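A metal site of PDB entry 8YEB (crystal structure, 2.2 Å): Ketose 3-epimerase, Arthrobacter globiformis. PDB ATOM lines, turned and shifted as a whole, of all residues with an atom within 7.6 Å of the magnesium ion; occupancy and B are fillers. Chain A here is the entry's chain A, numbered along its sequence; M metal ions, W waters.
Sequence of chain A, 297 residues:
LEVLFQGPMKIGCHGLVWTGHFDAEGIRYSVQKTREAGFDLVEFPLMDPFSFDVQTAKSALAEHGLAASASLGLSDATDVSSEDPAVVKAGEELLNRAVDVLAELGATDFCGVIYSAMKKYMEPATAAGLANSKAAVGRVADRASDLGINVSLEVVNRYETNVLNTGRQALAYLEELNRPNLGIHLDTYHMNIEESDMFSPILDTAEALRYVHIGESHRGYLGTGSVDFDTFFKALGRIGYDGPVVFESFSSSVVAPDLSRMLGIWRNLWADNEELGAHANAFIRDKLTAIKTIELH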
ATOM      1  N   HIS A  14     -28.902 -25.309  22.500  1.00  0.00           N
ATOM      2  CA  HIS A  14     -28.010 -24.525  23.331  1.00  0.00           C
ATOM      3  C   HIS A  14     -27.726 -25.324  24.608  1.00  0.00           C
ATOM      4  O   HIS A  14     -28.631 -25.955  25.133  1.00  0.00           O
ATOM      5  CB  HIS A  14     -28.624 -23.156  23.623  1.00  0.00           C
ATOM      6  CG  HIS A  14     -27.723 -22.190  24.288  1.00  0.00           C
ATOM      7  ND1 HIS A  14     -27.583 -22.080  25.658  1.00  0.00           N
ATOM      8  CD2 HIS A  14     -26.950 -21.222  23.762  1.00  0.00           C
ATOM      9  CE1 HIS A  14     -26.742 -21.067  25.939  1.00  0.00           C
ATOM     10  NE2 HIS A  14     -26.356 -20.524  24.804  1.00  0.00           N
ATOM     11  N   GLU A  43     -24.560 -26.386  20.975  1.00  0.00           N
ATOM     12  CA  GLU A  43     -23.846 -25.117  20.999  1.00  0.00           C
ATOM     13  C   GLU A  43     -23.325 -24.938  22.413  1.00  0.00           C
ATOM     14  O   GLU A  43     -24.119 -24.754  23.346  1.00  0.00           O
ATOM     15  CB  GLU A  43     -24.774 -23.974  20.618  1.00  0.00           C
ATOM     16  CG  GLU A  43     -24.177 -22.595  20.790  1.00  0.00           C
ATOM     17  CD  GLU A  43     -25.123 -21.466  20.384  1.00  0.00           C
ATOM     18  OE1 GLU A  43     -25.832 -21.618  19.344  1.00  0.00           O
ATOM     19  OE2 GLU A  43     -25.167 -20.460  21.088  1.00  0.00           O
ATOM     20  N   SER A  71     -20.646 -20.304  21.344  1.00  0.00           N
ATOM     21  CA  SER A  71     -21.179 -18.972  21.488  1.00  0.00           C
ATOM     22  C   SER A  71     -20.599 -18.409  22.766  1.00  0.00           C
ATOM     23  O   SER A  71     -20.216 -19.163  23.647  1.00  0.00           O
ATOM     24  CB  SER A  71     -22.706 -18.981  21.516  1.00  0.00           C
ATOM     25  OG  SER A  71     -23.179 -19.527  22.731  1.00  0.00           O
ATOM     26  N   GLY A 112     -22.495 -15.146  18.748  1.00  0.00           N
ATOM     27  CA  GLY A 112     -22.916 -14.538  19.993  1.00  0.00           C
ATOM     28  C   GLY A 112     -22.617 -13.039  20.032  1.00  0.00           C
ATOM     29  O   GLY A 112     -22.364 -12.415  19.004  1.00  0.00           O
ATOM     30  N   VAL A 113     -22.659 -12.478  21.239  1.00  0.00           N
ATOM     31  CA  VAL A 113     -22.472 -11.066  21.441  1.00  0.00           C
ATOM     32  C   VAL A 113     -20.992 -10.800  21.670  1.00  0.00           C
ATOM     33  O   VAL A 113     -20.547 -10.650  22.794  1.00  0.00           O
ATOM     34  CB  VAL A 113     -23.335 -10.527  22.592  1.00  0.00           C
ATOM     35  CG1 VAL A 113     -23.202  -9.014  22.705  1.00  0.00           C
ATOM     36  CG2 VAL A 113     -24.788 -10.929  22.419  1.00  0.00           C
ATOM     37  N   MET A 118     -22.281  -8.021  26.803  1.00  0.00           N
ATOM     38  CA  MET A 118     -23.653  -8.469  26.825  1.00  0.00           C
ATOM     39  C   MET A 118     -24.252  -8.010  28.136  1.00  0.00           C
ATOM     40  O   MET A 118     -24.165  -8.700  29.165  1.00  0.00           O
ATOM     41  CB  MET A 118     -23.738  -9.991  26.714  1.00  0.00           C
ATOM     42  CG  MET A 118     -25.114 -10.531  26.446  1.00  0.00           C
ATOM     43  SD  MET A 118     -25.031 -12.351  26.042  1.00  0.00           S
ATOM     44  CE  MET A 118     -24.519 -12.926  27.664  1.00  0.00           C
ATOM     45  N   GLU A 154     -24.347 -11.963  16.758  1.00  0.00           N
ATOM     46  CA  GLU A 154     -25.730 -12.165  17.152  1.00  0.00           C
ATOM     47  C   GLU A 154     -26.387 -10.842  17.526  1.00  0.00           C
ATOM     48  O   GLU A 154     -25.974 -10.176  18.467  1.00  0.00           O
ATOM     49  CB  GLU A 154     -25.827 -13.139  18.313  1.00  0.00           C
ATOM     50  CG  GLU A 154     -27.247 -13.507  18.632  1.00  0.00           C
ATOM     51  CD  GLU A 154     -27.403 -14.356  19.890  1.00  0.00           C
ATOM     52  OE1 GLU A 154     -26.407 -14.910  20.381  1.00  0.00           O
ATOM     53  OE2 GLU A 154     -28.521 -14.459  20.405  1.00  0.00           O
ATOM     54  N   VAL A 155     -27.454 -10.498  16.812  1.00  0.00           N
ATOM     55  CA  VAL A 155     -28.210  -9.301  17.079  1.00  0.00           C
ATOM     56  C   VAL A 155     -29.061  -9.533  18.313  1.00  0.00           C
ATOM     57  O   VAL A 155     -29.835 -10.494  18.356  1.00  0.00           O
ATOM     58  CB  VAL A 155     -29.085  -8.916  15.870  1.00  0.00           C
ATOM     59  CG1 VAL A 155     -29.919  -7.687  16.160  1.00  0.00           C
ATOM     60  CG2 VAL A 155     -28.229  -8.725  14.632  1.00  0.00           C
ATOM     61  N   VAL A 156     -28.926  -8.654  19.312  1.00  0.00           N
ATOM     62  CA  VAL A 156     -29.694  -8.821  20.544  1.00  0.00           C
ATOM     63  C   VAL A 156     -30.418  -7.526  20.912  1.00  0.00           C
ATOM     64  O   VAL A 156     -30.156  -6.450  20.352  1.00  0.00           O
ATOM     65  CB  VAL A 156     -28.811  -9.303  21.715  1.00  0.00           C
ATOM     66  CG1 VAL A 156     -28.223 -10.654  21.416  1.00  0.00           C
ATOM     67  CG2 VAL A 156     -27.688  -8.309  22.044  1.00  0.00           C
ATOM     68  N   GLU A 160     -29.477  -5.828  26.137  1.00  0.00           N
ATOM     69  CA  GLU A 160     -28.301  -6.697  26.149  1.00  0.00           C
ATOM     70  C   GLU A 160     -27.153  -6.097  25.346  1.00  0.00           C
ATOM     71  O   GLU A 160     -26.013  -6.562  25.453  1.00  0.00           O
ATOM     72  CB  GLU A 160     -28.660  -8.096  25.656  1.00  0.00           C
ATOM     73  CG  GLU A 160     -29.726  -8.759  26.522  1.00  0.00           C
ATOM     74  CD  GLU A 160     -29.742 -10.271  26.378  1.00  0.00           C
ATOM     75  OE1 GLU A 160     -28.761 -10.798  25.835  1.00  0.00           O
ATOM     76  OE2 GLU A 160     -30.744 -10.890  26.739  1.00  0.00           O
ATOM     77  N   HIS A 185     -26.069 -13.310  12.927  1.00  0.00           N
ATOM     78  CA  HIS A 185     -26.786 -14.326  13.684  1.00  0.00           C
ATOM     79  C   HIS A 185     -28.073 -13.684  14.221  1.00  0.00           C
ATOM     80  O   HIS A 185     -28.029 -12.785  15.055  1.00  0.00           O
ATOM     81  CB  HIS A 185     -25.857 -14.861  14.780  1.00  0.00           C
ATOM     82  CG  HIS A 185     -26.509 -15.708  15.810  1.00  0.00           C
ATOM     83  ND1 HIS A 185     -25.894 -16.012  17.012  1.00  0.00           N
ATOM     84  CD2 HIS A 185     -27.709 -16.302  15.828  1.00  0.00           C
ATOM     85  CE1 HIS A 185     -26.715 -16.763  17.741  1.00  0.00           C
ATOM     86  NE2 HIS A 185     -27.815 -16.956  17.050  1.00  0.00           N
ATOM     87  N   LEU A 186     -29.205 -14.205  13.794  1.00  0.00           N
ATOM     88  CA  LEU A 186     -30.507 -13.718  14.273  1.00  0.00           C
ATOM     89  C   LEU A 186     -31.111 -14.687  15.282  1.00  0.00           C
ATOM     90  O   LEU A 186     -30.970 -15.913  15.168  1.00  0.00           O
ATOM     91  CB  LEU A 186     -31.482 -13.578  13.089  1.00  0.00           C
ATOM     92  CG  LEU A 186     -31.234 -12.415  12.136  1.00  0.00           C
ATOM     93  CD1 LEU A 186     -32.310 -12.375  11.066  1.00  0.00           C
ATOM     94  CD2 LEU A 186     -31.165 -11.102  12.889  1.00  0.00           C
ATOM     95  N   ASP A 187     -31.826 -14.101  16.243  1.00  0.00           N
ATOM     96  CA  ASP A 187     -32.477 -14.823  17.303  1.00  0.00           C
ATOM     97  C   ASP A 187     -33.913 -14.337  17.385  1.00  0.00           C
ATOM     98  O   ASP A 187     -34.160 -13.144  17.525  1.00  0.00           O
ATOM     99  CB  ASP A 187     -31.738 -14.563  18.614  1.00  0.00           C
ATOM    100  CG  ASP A 187     -32.310 -15.314  19.790  1.00  0.00           C
ATOM    101  OD1 ASP A 187     -33.550 -15.493  19.863  1.00  0.00           O
ATOM    102  OD2 ASP A 187     -31.517 -15.696  20.647  1.00  0.00           O
ATOM    103  N   THR A 188     -34.867 -15.269  17.338  1.00  0.00           N
ATOM    104  CA  THR A 188     -36.274 -14.918  17.278  1.00  0.00           C
ATOM    105  C   THR A 188     -36.708 -14.176  18.543  1.00  0.00           C
ATOM    106  O   THR A 188     -37.574 -13.308  18.479  1.00  0.00           O
ATOM    107  CB  THR A 188     -37.164 -16.157  17.083  1.00  0.00           C
ATOM    108  OG1 THR A 188     -36.948 -17.092  18.142  1.00  0.00           O
ATOM    109  CG2 THR A 188     -36.930 -16.818  15.745  1.00  0.00           C
ATOM    110  N   TYR A 189     -36.135 -14.541  19.693  1.00  0.00           N
ATOM    111  CA  TYR A 189     -36.452 -13.869  20.944  1.00  0.00           C
ATOM    112  C   TYR A 189     -36.093 -12.378  20.849  1.00  0.00           C
ATOM    113  O   TYR A 189     -36.880 -11.525  21.247  1.00  0.00           O
ATOM    114  CB  TYR A 189     -35.691 -14.539  22.083  1.00  0.00           C
ATOM    115  CG  TYR A 189     -35.585 -13.731  23.356  1.00  0.00           C
ATOM    116  CD1 TYR A 189     -36.672 -13.598  24.194  1.00  0.00           C
ATOM    117  CD2 TYR A 189     -34.412 -13.090  23.692  1.00  0.00           C
ATOM    118  CE1 TYR A 189     -36.590 -12.847  25.352  1.00  0.00           C
ATOM    119  CE2 TYR A 189     -34.313 -12.340  24.846  1.00  0.00           C
ATOM    120  CZ  TYR A 189     -35.402 -12.219  25.676  1.00  0.00           C
ATOM    121  OH  TYR A 189     -35.318 -11.481  26.841  1.00  0.00           O
ATOM    122  N   HIS A 190     -34.896 -12.072  20.343  1.00  0.00           N
ATOM    123  CA  HIS A 190     -34.457 -10.689  20.234  1.00  0.00           C
ATOM    124  C   HIS A 190     -35.202  -9.952  19.132  1.00  0.00           C
ATOM    125  O   HIS A 190     -35.492  -8.766  19.268  1.00  0.00           O
ATOM    126  CB  HIS A 190     -32.931 -10.627  20.019  1.00  0.00           C
ATOM    127  CG  HIS A 190     -32.159 -11.222  21.131  1.00  0.00           C
ATOM    128  ND1 HIS A 190     -32.074 -10.599  22.368  1.00  0.00           N
ATOM    129  CD2 HIS A 190     -31.442 -12.372  21.237  1.00  0.00           C
ATOM    130  CE1 HIS A 190     -31.310 -11.346  23.178  1.00  0.00           C
ATOM    131  NE2 HIS A 190     -30.927 -12.426  22.512  1.00  0.00           N
ATOM    132  N   TYR A 211     -26.286 -17.777  11.014  1.00  0.00           N
ATOM    133  CA  TYR A 211     -26.629 -18.525  12.218  1.00  0.00           C
ATOM    134  C   TYR A 211     -27.996 -18.113  12.724  1.00  0.00           C
ATOM    135  O   TYR A 211     -28.350 -16.939  12.685  1.00  0.00           O
ATOM    136  CB  TYR A 211     -25.568 -18.308  13.302  1.00  0.00           C
ATOM    137  CG  TYR A 211     -25.442 -19.419  14.314  1.00  0.00           C
ATOM    138  CD1 TYR A 211     -26.280 -19.491  15.416  1.00  0.00           C
ATOM    139  CD2 TYR A 211     -24.451 -20.383  14.192  1.00  0.00           C
ATOM    140  CE1 TYR A 211     -26.139 -20.486  16.351  1.00  0.00           C
ATOM    141  CE2 TYR A 211     -24.286 -21.383  15.127  1.00  0.00           C
ATOM    142  CZ  TYR A 211     -25.140 -21.433  16.214  1.00  0.00           C
ATOM    143  OH  TYR A 211     -24.997 -22.417  17.156  1.00  0.00           O
ATOM    144  N   VAL A 212     -28.763 -19.070  13.270  1.00  0.00           N
ATOM    145  CA  VAL A 212     -30.120 -18.815  13.741  1.00  0.00           C
ATOM    146  C   VAL A 212     -30.381 -19.405  15.125  1.00  0.00           C
ATOM    147  O   VAL A 212     -30.107 -20.571  15.383  1.00  0.00           O
ATOM    148  CB  VAL A 212     -31.147 -19.307  12.717  1.00  0.00           C
ATOM    149  CG1 VAL A 212     -32.547 -19.402  13.292  1.00  0.00           C
ATOM    150  CG2 VAL A 212     -31.157 -18.413  11.484  1.00  0.00           C
ATOM    151  N   HIS A 213     -30.928 -18.588  16.028  1.00  0.00           N
ATOM    152  CA  HIS A 213     -31.394 -19.070  17.313  1.00  0.00           C
ATOM    153  C   HIS A 213     -32.916 -19.094  17.338  1.00  0.00           C
ATOM    154  O   HIS A 213     -33.563 -18.121  16.975  1.00  0.00           O
ATOM    155  CB  HIS A 213     -30.879 -18.182  18.462  1.00  0.00           C
ATOM    156  CG  HIS A 213     -29.613 -18.653  19.071  1.00  0.00           C
ATOM    157  ND1 HIS A 213     -28.952 -17.902  20.025  1.00  0.00           N
ATOM    158  CD2 HIS A 213     -28.878 -19.752  18.882  1.00  0.00           C
ATOM    159  CE1 HIS A 213     -27.847 -18.559  20.385  1.00  0.00           C
ATOM    160  NE2 HIS A 213     -27.791 -19.682  19.700  1.00  0.00           N
ATOM    161  N   ILE A 214     -33.486 -20.212  17.792  1.00  0.00           N
ATOM    162  CA  ILE A 214     -34.914 -20.364  17.924  1.00  0.00           C
ATOM    163  C   ILE A 214     -35.283 -20.229  19.401  1.00  0.00           C
ATOM    164  O   ILE A 214     -35.054 -21.156  20.193  1.00  0.00           O
ATOM    165  CB  ILE A 214     -35.362 -21.720  17.362  1.00  0.00           C
ATOM    166  CG1 ILE A 214     -35.044 -21.845  15.870  1.00  0.00           C
ATOM    167  CG2 ILE A 214     -36.844 -21.966  17.626  1.00  0.00           C
ATOM    168  CD1 ILE A 214     -35.623 -20.727  15.044  1.00  0.00           C
ATOM    169  N   GLY A 215     -35.925 -19.117  19.741  1.00  0.00           N
ATOM    170  CA  GLY A 215     -36.348 -18.860  21.109  1.00  0.00           C
ATOM    171  C   GLY A 215     -37.720 -18.184  21.209  1.00  0.00           C
ATOM    172  O   GLY A 215     -38.033 -17.255  20.461  1.00  0.00           O
ATOM    173  N   ARG A 219     -38.438 -17.031  26.431  1.00  0.00           N
ATOM    174  CA  ARG A 219     -37.325 -17.973  26.388  1.00  0.00           C
ATOM    175  C   ARG A 219     -37.654 -19.338  27.004  1.00  0.00           C
ATOM    176  O   ARG A 219     -36.734 -20.045  27.410  1.00  0.00           O
ATOM    177  CB  ARG A 219     -36.041 -17.392  26.984  1.00  0.00           C
ATOM    178  CG  ARG A 219     -35.780 -15.942  26.583  1.00  0.00           C
ATOM    179  CD  ARG A 219     -34.370 -15.491  26.821  1.00  0.00           C
ATOM    180  NE  ARG A 219     -33.526 -15.818  25.690  1.00  0.00           N
ATOM    181  CZ  ARG A 219     -32.371 -15.212  25.412  1.00  0.00           C
ATOM    182  NH1 ARG A 219     -31.714 -15.527  24.324  1.00  0.00           N
ATOM    183  NH2 ARG A 219     -31.895 -14.254  26.188  1.00  0.00           N
ATOM    184  N   VAL A 246     -30.630 -23.367  15.907  1.00  0.00           N
ATOM    185  CA  VAL A 246     -30.380 -23.827  17.261  1.00  0.00           C
ATOM    186  C   VAL A 246     -31.418 -23.319  18.244  1.00  0.00           C
ATOM    187  O   VAL A 246     -31.626 -22.115  18.396  1.00  0.00           O
ATOM    188  CB  VAL A 246     -28.972 -23.420  17.739  1.00  0.00           C
ATOM    189  CG1 VAL A 246     -28.650 -24.080  19.067  1.00  0.00           C
ATOM    190  CG2 VAL A 246     -27.924 -23.769  16.706  1.00  0.00           C
ATOM    191  N   GLU A 248     -32.799 -22.361  21.810  1.00  0.00           N
ATOM    192  CA  GLU A 248     -32.219 -21.747  22.996  1.00  0.00           C
ATOM    193  C   GLU A 248     -33.325 -21.423  23.991  1.00  0.00           C
ATOM    194  O   GLU A 248     -34.313 -20.797  23.650  1.00  0.00           O
ATOM    195  CB  GLU A 248     -31.478 -20.462  22.581  1.00  0.00           C
ATOM    196  CG  GLU A 248     -30.690 -19.830  23.700  1.00  0.00           C
ATOM    197  CD  GLU A 248     -29.999 -18.545  23.298  1.00  0.00           C
ATOM    198  OE1 GLU A 248     -28.818 -18.400  23.635  1.00  0.00           O
ATOM    199  OE2 GLU A 248     -30.626 -17.710  22.605  1.00  0.00           O
ATOM    200  N   PHE A 250     -34.041 -20.723  28.493  1.00  0.00           N
ATOM    201  CA  PHE A 250     -33.468 -20.505  29.808  1.00  0.00           C
ATOM    202  C   PHE A 250     -34.558 -20.551  30.884  1.00  0.00           C
ATOM    203  O   PHE A 250     -35.616 -19.938  30.750  1.00  0.00           O
ATOM    204  CB  PHE A 250     -32.743 -19.163  29.900  1.00  0.00           C
ATOM    205  CG  PHE A 250     -31.648 -18.991  28.890  1.00  0.00           C
ATOM    206  CD1 PHE A 250     -30.388 -19.500  29.139  1.00  0.00           C
ATOM    207  CD2 PHE A 250     -31.874 -18.333  27.698  1.00  0.00           C
ATOM    208  CE1 PHE A 250     -29.374 -19.372  28.206  1.00  0.00           C
ATOM    209  CE2 PHE A 250     -30.866 -18.189  26.768  1.00  0.00           C
ATOM    210  CZ  PHE A 250     -29.613 -18.715  27.032  1.00  0.00           C
ATOM    211  N   LEU A 263     -28.634 -12.519  31.766  1.00  0.00           N
ATOM    212  CA  LEU A 263     -29.812 -12.593  30.898  1.00  0.00           C
ATOM    213  C   LEU A 263     -31.107 -12.383  31.671  1.00  0.00           C
ATOM    214  O   LEU A 263     -32.178 -12.403  31.073  1.00  0.00           O
ATOM    215  CB  LEU A 263     -29.850 -13.936  30.171  1.00  0.00           C
ATOM    216  CG  LEU A 263     -28.626 -14.278  29.305  1.00  0.00           C
ATOM    217  CD1 LEU A 263     -28.839 -15.577  28.553  1.00  0.00           C
ATOM    218  CD2 LEU A 263     -28.313 -13.161  28.354  1.00  0.00           C
HETATM  219 MG    MG M   1     -29.500 -16.093  21.342  1.00  0.00          MG
HETATM  220  O   HOH W   1     -28.114 -15.872  22.729  1.00  0.00           O
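Arg 219 touches the magnesium ion.
Of the 26 residues printed, 5 come within 4 Å of the magnesium ion.
Water W1 binds the magnesium ion.
The magnesium ion is bound by OE2 of Glu 154 (2.1 Å).
The magnesium ion is bound by OD2 of Asp 187 (2.2 Å).
The magnesium ion is bound by ND1 of His 213 (2.3 Å).
OE2 of Glu 248 is bound to the magnesium ion (2.3 Å).
Water W1 lies within hydrogen-bond range of the side-chain carboxylate of Glu 248 and the side-chain carboxylate of Glu 154.
ND1 of His 213 sits close to NE2 of His 185.
N of Tyr 189 sits at hydrogen-bond distance from OD1 of Asp 187 (2.8 Å).
O of His 213 lies within hydrogen-bond range of N of Thr 188, at 3.2 Å.
A ring nitrogen (NE2) of His 14 lies close to the side-chain carboxylate (OE1) of Glu 248 (3.5 Å).
The backbone carbonyl oxygen (O) of Leu 186 sits at hydrogen-bond distance from the backbone NH (N) of His 213, 2.8 Å away.
The side-chain carboxylate (OD2) of Asp 187 lies close to the guanidinium group (NH1) of Arg 219.
O of Gly 112 is in hydrogen-bond range of N of Glu 154, 3.0 Å away.
The backbone carbonyl oxygen (O) of Arg 219 sits at hydrogen-bond distance from the backbone NH (N) of Phe 250.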
